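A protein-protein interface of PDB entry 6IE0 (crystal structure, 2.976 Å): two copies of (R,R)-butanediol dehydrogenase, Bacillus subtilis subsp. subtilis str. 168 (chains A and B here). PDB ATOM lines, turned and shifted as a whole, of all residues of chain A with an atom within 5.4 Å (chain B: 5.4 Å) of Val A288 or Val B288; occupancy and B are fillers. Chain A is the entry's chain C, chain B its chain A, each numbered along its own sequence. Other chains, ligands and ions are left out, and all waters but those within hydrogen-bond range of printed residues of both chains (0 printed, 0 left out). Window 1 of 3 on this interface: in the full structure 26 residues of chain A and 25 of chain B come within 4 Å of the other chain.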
ATOM      1  N   LEU A 251       0.466  17.121 -21.756  1.00  0.00           N
ATOM      2  CA  LEU A 251      -0.182  15.863 -22.113  1.00  0.00           C
ATOM      3  C   LEU A 251       0.439  14.700 -21.352  1.00  0.00           C
ATOM      4  O   LEU A 251      -0.264  13.771 -20.934  1.00  0.00           O
ATOM      5  CB  LEU A 251      -0.098  15.627 -23.621  1.00  0.00           C
ATOM      6  CG  LEU A 251      -0.799  14.366 -24.144  1.00  0.00           C
ATOM      7  CD1 LEU A 251      -2.269  14.344 -23.742  1.00  0.00           C
ATOM      8  CD2 LEU A 251      -0.655  14.245 -25.653  1.00  0.00           C
ATOM      9  N   ILE A 255      -1.766  12.345 -18.495  1.00  0.00           N
ATOM     10  CA  ILE A 255      -1.789  10.888 -18.481  1.00  0.00           C
ATOM     11  C   ILE A 255      -1.257  10.362 -17.156  1.00  0.00           C
ATOM     12  O   ILE A 255      -1.820   9.427 -16.571  1.00  0.00           O
ATOM     13  CB  ILE A 255      -0.992  10.334 -19.677  1.00  0.00           C
ATOM     14  CG1 ILE A 255      -1.646  10.761 -20.993  1.00  0.00           C
ATOM     15  CG2 ILE A 255      -0.886   8.821 -19.601  1.00  0.00           C
ATOM     16  CD1 ILE A 255      -0.819  10.446 -22.214  1.00  0.00           C
ATOM     17  N   GLU A 263      -8.392   7.526 -17.594  1.00  0.00           N
ATOM     18  CA  GLU A 263      -8.662   7.976 -18.954  1.00  0.00           C
ATOM     19  C   GLU A 263      -8.213   9.420 -19.125  1.00  0.00           C
ATOM     20  O   GLU A 263      -8.507  10.269 -18.279  1.00  0.00           O
ATOM     21  CB  GLU A 263     -10.151   7.846 -19.289  1.00  0.00           C
ATOM     22  CG  GLU A 263     -10.480   8.040 -20.763  1.00  0.00           C
ATOM     23  CD  GLU A 263     -11.924   7.697 -21.092  1.00  0.00           C
ATOM     24  OE1 GLU A 263     -12.153   6.754 -21.880  1.00  0.00           O
ATOM     25  OE2 GLU A 263     -12.830   8.371 -20.558  1.00  0.00           O
ATOM     26  N   THR A 264      -7.499   9.691 -20.214  1.00  0.00           N
ATOM     27  CA  THR A 264      -7.089  11.041 -20.581  1.00  0.00           C
ATOM     28  C   THR A 264      -7.832  11.452 -21.844  1.00  0.00           C
ATOM     29  O   THR A 264      -7.665  10.824 -22.897  1.00  0.00           O
ATOM     30  CB  THR A 264      -5.580  11.123 -20.800  1.00  0.00           C
ATOM     31  OG1 THR A 264      -4.902  10.596 -19.652  1.00  0.00           O
ATOM     32  CG2 THR A 264      -5.155  12.565 -21.015  1.00  0.00           C
ATOM     33  N   ILE A 266      -8.357  14.173 -24.672  1.00  0.00           N
ATOM     34  CA  ILE A 266      -7.682  15.297 -25.313  1.00  0.00           C
ATOM     35  C   ILE A 266      -8.729  16.225 -25.919  1.00  0.00           C
ATOM     36  O   ILE A 266      -9.499  15.822 -26.799  1.00  0.00           O
ATOM     37  CB  ILE A 266      -6.695  14.816 -26.385  1.00  0.00           C
ATOM     38  CG1 ILE A 266      -5.709  13.808 -25.791  1.00  0.00           C
ATOM     39  CG2 ILE A 266      -5.953  16.000 -26.986  1.00  0.00           C
ATOM     40  CD1 ILE A 266      -4.698  13.290 -26.793  1.00  0.00           C
ATOM     41  N   ILE A 281       1.248   4.676 -20.341  1.00  0.00           N
ATOM     42  CA  ILE A 281      -0.044   4.110 -20.704  1.00  0.00           C
ATOM     43  C   ILE A 281      -0.090   2.623 -20.374  1.00  0.00           C
ATOM     44  O   ILE A 281      -1.120   2.103 -19.931  1.00  0.00           O
ATOM     45  CB  ILE A 281      -0.332   4.381 -22.193  1.00  0.00           C
ATOM     46  CG1 ILE A 281      -0.381   5.888 -22.458  1.00  0.00           C
ATOM     47  CG2 ILE A 281      -1.637   3.720 -22.625  1.00  0.00           C
ATOM     48  CD1 ILE A 281      -0.532   6.252 -23.922  1.00  0.00           C
ATOM     49  N   ARG A 286      -3.797   2.472 -18.815  1.00  0.00           N
ATOM     50  CA  ARG A 286      -4.500   3.731 -18.988  1.00  0.00           C
ATOM     51  C   ARG A 286      -5.115   3.812 -20.383  1.00  0.00           C
ATOM     52  O   ARG A 286      -4.950   2.923 -21.222  1.00  0.00           O
ATOM     53  CB  ARG A 286      -3.558   4.904 -18.725  1.00  0.00           C
ATOM     54  CG  ARG A 286      -3.304   5.157 -17.249  1.00  0.00           C
ATOM     55  CD  ARG A 286      -2.076   6.020 -17.030  1.00  0.00           C
ATOM     56  NE  ARG A 286      -1.907   6.366 -15.621  1.00  0.00           N
ATOM     57  CZ  ARG A 286      -0.732   6.421 -15.000  1.00  0.00           C
ATOM     58  NH1 ARG A 286       0.382   6.154 -15.665  1.00  0.00           N
ATOM     59  NH2 ARG A 286      -0.672   6.746 -13.716  1.00  0.00           N
ATOM     60  N   THR A 287      -5.849   4.894 -20.623  1.00  0.00           N
ATOM     61  CA  THR A 287      -6.536   5.123 -21.883  1.00  0.00           C
ATOM     62  C   THR A 287      -6.409   6.593 -22.249  1.00  0.00           C
ATOM     63  O   THR A 287      -6.592   7.471 -21.403  1.00  0.00           O
ATOM     64  CB  THR A 287      -8.019   4.720 -21.795  1.00  0.00           C
ATOM     65  OG1 THR A 287      -8.125   3.295 -21.671  1.00  0.00           O
ATOM     66  CG2 THR A 287      -8.791   5.181 -23.024  1.00  0.00           C
ATOM     67  N   VAL A 288      -6.101   6.859 -23.513  1.00  0.00           N
ATOM     68  CA  VAL A 288      -6.113   8.209 -24.063  1.00  0.00           C
ATOM     69  C   VAL A 288      -7.165   8.238 -25.159  1.00  0.00           C
ATOM     70  O   VAL A 288      -7.223   7.329 -25.994  1.00  0.00           O
ATOM     71  CB  VAL A 288      -4.732   8.628 -24.599  1.00  0.00           C
ATOM     72  CG1 VAL A 288      -4.762  10.066 -25.085  1.00  0.00           C
ATOM     73  CG2 VAL A 288      -3.678   8.464 -23.511  1.00  0.00           C
ATOM     74  N   LYS A 289      -7.998   9.274 -25.152  1.00  0.00           N
ATOM     75  CA  LYS A 289      -9.201   9.322 -25.974  1.00  0.00           C
ATOM     76  C   LYS A 289      -9.291  10.661 -26.688  1.00  0.00           C
ATOM     77  O   LYS A 289      -9.107  11.716 -26.068  1.00  0.00           O
ATOM     78  CB  LYS A 289     -10.444   9.100 -25.103  1.00  0.00           C
ATOM     79  CG  LYS A 289     -11.748   8.951 -25.854  1.00  0.00           C
ATOM     80  CD  LYS A 289     -12.893   8.730 -24.879  1.00  0.00           C
ATOM     81  CE  LYS A 289     -14.074   8.076 -25.570  1.00  0.00           C
ATOM     82  NZ  LYS A 289     -14.144   8.467 -27.005  1.00  0.00           N
ATOM     83  N   GLY A 290      -9.575  10.617 -27.985  1.00  0.00           N
ATOM     84  CA  GLY A 290      -9.754  11.820 -28.786  1.00  0.00           C
ATOM     85  C   GLY A 290     -11.211  12.205 -28.893  1.00  0.00           C
ATOM     86  O   GLY A 290     -12.092  11.349 -29.022  1.00  0.00           O
ATOM     87  N   LEU B 251       4.431   3.414 -33.503  1.00  0.00           N
ATOM     88  CA  LEU B 251       3.266   3.761 -32.694  1.00  0.00           C
ATOM     89  C   LEU B 251       2.420   4.819 -33.393  1.00  0.00           C
ATOM     90  O   LEU B 251       1.184   4.765 -33.355  1.00  0.00           O
ATOM     91  CB  LEU B 251       3.711   4.251 -31.315  1.00  0.00           C
ATOM     92  CG  LEU B 251       2.786   4.193 -30.082  1.00  0.00           C
ATOM     93  CD1 LEU B 251       2.792   5.515 -29.344  1.00  0.00           C
ATOM     94  CD2 LEU B 251       1.351   3.773 -30.393  1.00  0.00           C
ATOM     95  N   ILE B 255      -1.667   4.174 -34.824  1.00  0.00           N
ATOM     96  CA  ILE B 255      -2.799   5.067 -34.607  1.00  0.00           C
ATOM     97  C   ILE B 255      -3.367   5.535 -35.940  1.00  0.00           C
ATOM     98  O   ILE B 255      -4.588   5.597 -36.124  1.00  0.00           O
ATOM     99  CB  ILE B 255      -2.386   6.257 -33.721  1.00  0.00           C
ATOM    100  CG1 ILE B 255      -1.941   5.773 -32.338  1.00  0.00           C
ATOM    101  CG2 ILE B 255      -3.531   7.253 -33.598  1.00  0.00           C
ATOM    102  CD1 ILE B 255      -1.234   6.827 -31.522  1.00  0.00           C
ATOM    103  N   GLU B 263      -9.169   1.880 -32.302  1.00  0.00           N
ATOM    104  CA  GLU B 263      -8.461   1.691 -31.041  1.00  0.00           C
ATOM    105  C   GLU B 263      -7.065   1.156 -31.315  1.00  0.00           C
ATOM    106  O   GLU B 263      -6.901   0.212 -32.093  1.00  0.00           O
ATOM    107  CB  GLU B 263      -9.218   0.733 -30.117  1.00  0.00           C
ATOM    108  CG  GLU B 263      -8.625   0.601 -28.721  1.00  0.00           C
ATOM    109  CD  GLU B 263      -9.489  -0.244 -27.797  1.00  0.00           C
ATOM    110  OE1 GLU B 263     -10.014   0.301 -26.802  1.00  0.00           O
ATOM    111  OE2 GLU B 263      -9.646  -1.454 -28.065  1.00  0.00           O
ATOM    112  N   THR B 264      -6.069   1.755 -30.670  1.00  0.00           N
ATOM    113  CA  THR B 264      -4.685   1.302 -30.741  1.00  0.00           C
ATOM    114  C   THR B 264      -4.291   0.732 -29.384  1.00  0.00           C
ATOM    115  O   THR B 264      -4.290   1.452 -28.379  1.00  0.00           O
ATOM    116  CB  THR B 264      -3.752   2.444 -31.146  1.00  0.00           C
ATOM    117  OG1 THR B 264      -4.235   3.052 -32.350  1.00  0.00           O
ATOM    118  CG2 THR B 264      -2.341   1.923 -31.383  1.00  0.00           C
ATOM    119  N   ILE B 266      -1.464  -0.818 -27.079  1.00  0.00           N
ATOM    120  CA  ILE B 266      -0.012  -0.872 -26.943  1.00  0.00           C
ATOM    121  C   ILE B 266       0.350  -2.147 -26.193  1.00  0.00           C
ATOM    122  O   ILE B 266      -0.028  -2.325 -25.030  1.00  0.00           O
ATOM    123  CB  ILE B 266       0.532   0.366 -26.217  1.00  0.00           C
ATOM    124  CG1 ILE B 266       0.096   1.646 -26.928  1.00  0.00           C
ATOM    125  CG2 ILE B 266       2.045   0.312 -26.149  1.00  0.00           C
ATOM    126  CD1 ILE B 266       0.627   2.909 -26.274  1.00  0.00           C
ATOM    127  N   ILE B 281      -5.087  11.501 -32.933  1.00  0.00           N
ATOM    128  CA  ILE B 281      -6.051  10.919 -32.007  1.00  0.00           C
ATOM    129  C   ILE B 281      -7.347  11.720 -32.006  1.00  0.00           C
ATOM    130  O   ILE B 281      -8.441  11.150 -31.953  1.00  0.00           O
ATOM    131  CB  ILE B 281      -5.443  10.831 -30.595  1.00  0.00           C
ATOM    132  CG1 ILE B 281      -4.226   9.905 -30.583  1.00  0.00           C
ATOM    133  CG2 ILE B 281      -6.481  10.348 -29.588  1.00  0.00           C
ATOM    134  CD1 ILE B 281      -3.479   9.902 -29.260  1.00  0.00           C
ATOM    135  N   ARG B 286     -10.125   8.807 -31.956  1.00  0.00           N
ATOM    136  CA  ARG B 286      -9.465   7.528 -31.765  1.00  0.00           C
ATOM    137  C   ARG B 286      -9.196   7.275 -30.284  1.00  0.00           C
ATOM    138  O   ARG B 286      -9.447   8.117 -29.419  1.00  0.00           O
ATOM    139  CB  ARG B 286      -8.179   7.475 -32.582  1.00  0.00           C
ATOM    140  CG  ARG B 286      -8.415   7.310 -34.071  1.00  0.00           C
ATOM    141  CD  ARG B 286      -7.104   7.307 -34.827  1.00  0.00           C
ATOM    142  NE  ARG B 286      -7.273   6.885 -36.212  1.00  0.00           N
ATOM    143  CZ  ARG B 286      -6.894   7.609 -37.261  1.00  0.00           C
ATOM    144  NH1 ARG B 286      -6.325   8.790 -37.076  1.00  0.00           N
ATOM    145  NH2 ARG B 286      -7.082   7.150 -38.491  1.00  0.00           N
ATOM    146  N   THR B 287      -8.679   6.085 -29.996  1.00  0.00           N
ATOM    147  CA  THR B 287      -8.408   5.649 -28.637  1.00  0.00           C
ATOM    148  C   THR B 287      -7.092   4.886 -28.611  1.00  0.00           C
ATOM    149  O   THR B 287      -6.808   4.091 -29.511  1.00  0.00           O
ATOM    150  CB  THR B 287      -9.547   4.767 -28.101  1.00  0.00           C
ATOM    151  OG1 THR B 287     -10.774   5.508 -28.125  1.00  0.00           O
ATOM    152  CG2 THR B 287      -9.264   4.316 -26.675  1.00  0.00           C
ATOM    153  N   VAL B 288      -6.281   5.154 -27.593  1.00  0.00           N
ATOM    154  CA  VAL B 288      -5.074   4.387 -27.324  1.00  0.00           C
ATOM    155  C   VAL B 288      -5.232   3.745 -25.954  1.00  0.00           C
ATOM    156  O   VAL B 288      -5.654   4.407 -24.999  1.00  0.00           O
ATOM    157  CB  VAL B 288      -3.812   5.267 -27.386  1.00  0.00           C
ATOM    158  CG1 VAL B 288      -2.563   4.405 -27.334  1.00  0.00           C
ATOM    159  CG2 VAL B 288      -3.828   6.114 -28.650  1.00  0.00           C
ATOM    160  N   LYS B 289      -4.898   2.461 -25.860  1.00  0.00           N
ATOM    161  CA  LYS B 289      -5.181   1.662 -24.675  1.00  0.00           C
ATOM    162  C   LYS B 289      -3.931   0.899 -24.265  1.00  0.00           C
ATOM    163  O   LYS B 289      -3.273   0.279 -25.109  1.00  0.00           O
ATOM    164  CB  LYS B 289      -6.337   0.690 -24.934  1.00  0.00           C
ATOM    165  CG  LYS B 289      -6.784  -0.093 -23.714  1.00  0.00           C
ATOM    166  CD  LYS B 289      -7.814  -1.146 -24.090  1.00  0.00           C
ATOM    167  CE  LYS B 289      -9.230  -0.676 -23.786  1.00  0.00           C
ATOM    168  NZ  LYS B 289      -9.699  -1.124 -22.445  1.00  0.00           N
ATOM    169  N   GLY B 290      -3.616   0.937 -22.972  1.00  0.00           N
ATOM    170  CA  GLY B 290      -2.471   0.215 -22.447  1.00  0.00           C
ATOM    171  C   GLY B 290      -2.875  -1.155 -21.929  1.00  0.00           C
ATOM    172  O   GLY B 290      -3.948  -1.328 -21.354  1.00  0.00           O
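Val A288 touches two residues of chain B.
Of the printed residues of chain B, Ile A281 touches Lys B289 and Gly B290.
Of the printed residues of chain A, Thr B287 touches Thr A287 (3.8 Å) and Val A288 (3.3 Å).
Printed residues of chain A within 4 Å of Lys B289: Ile A281 and Arg A286.
Of the printed residues of chain B, Arg A286 touches Lys B289 and Gly B290.
Printed residues of chain B within 4 Å of Gly A290: Ile B281 and Arg B286.
Glu A263 touches none of the printed residues of chain B.
Leu B251 touches none of the printed residues of chain A.
The nearest residue of chain A that does not touch Val B288 is Arg A286 (4.1 Å).
The backbone NH of Gly A290 lies within hydrogen-bond range of the backbone carbonyl oxygen of Arg B286 (2.9 Å).
N of Val B288 is in hydrogen-bond range of O of Val A288, 2.9 Å away.
N of Gly B290 sits at hydrogen-bond distance from O of Arg A286 (3.0 Å).
Arg A286 touches Lys B289, and with the chains exchanged Lys A289 touches Arg B286.
Arg A286 touches Gly B290, and with the chains exchanged Gly A290 touches Arg B286.
Thr A287 touches its own counterpart, Thr B287.
Val B288 touches its own counterpart, Val A288.
11 positions are printed for both chains.
Printed residues of chain B that touch a printed residue of chain A: Ile B281, Arg B286, Thr B287, Val B288, Lys B289 and Gly B290.
Among the printed residues, 11 pairs touch across the chains.
Among the printed residues, no Asp or Glu carboxylate lies within 4 Å of a Lys or Arg side-chain nitrogen of the other chain.
C of Lys B289 touches CG2 of Ile A281, at 3.99 Å.
O of Ile A281 touches CA of Gly B290, at 3.4 Å.
Arg A286 touches Lys B289 (O to CA, 3.7 Å).
Thr B287 touches Thr A287.
Thr A287 touches Val B288 (CA to O, 3.3 Å).
Thr B287 touches Val A288.
CA of Lys A289 touches O of Arg B286 (3.7 Å).
Ile B281 touches Gly A290.
The backbone carbonyl oxygen of Ile B255 is in hydrogen-bond range of the guanidinium group of Arg B286 (3.0 Å).
The backbone carbonyl oxygen of Lys B289 is in hydrogen-bond range of the backbone NH of Ile B266 (2.9 Å).
The backbone NH (N) of Arg B286 sits at hydrogen-bond distance from the backbone carbonyl oxygen (O) of Ile B281 (2.9 Å).
N of Thr A264 is in hydrogen-bond range of O of Thr A287, 2.7 Å away.
The backbone NH (N) of Ile A266 sits at hydrogen-bond distance from the backbone carbonyl oxygen (O) of Lys A289, 2.9 Å away.
O of Ile A281 lies within hydrogen-bond range of N of Arg A286 (2.9 Å).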
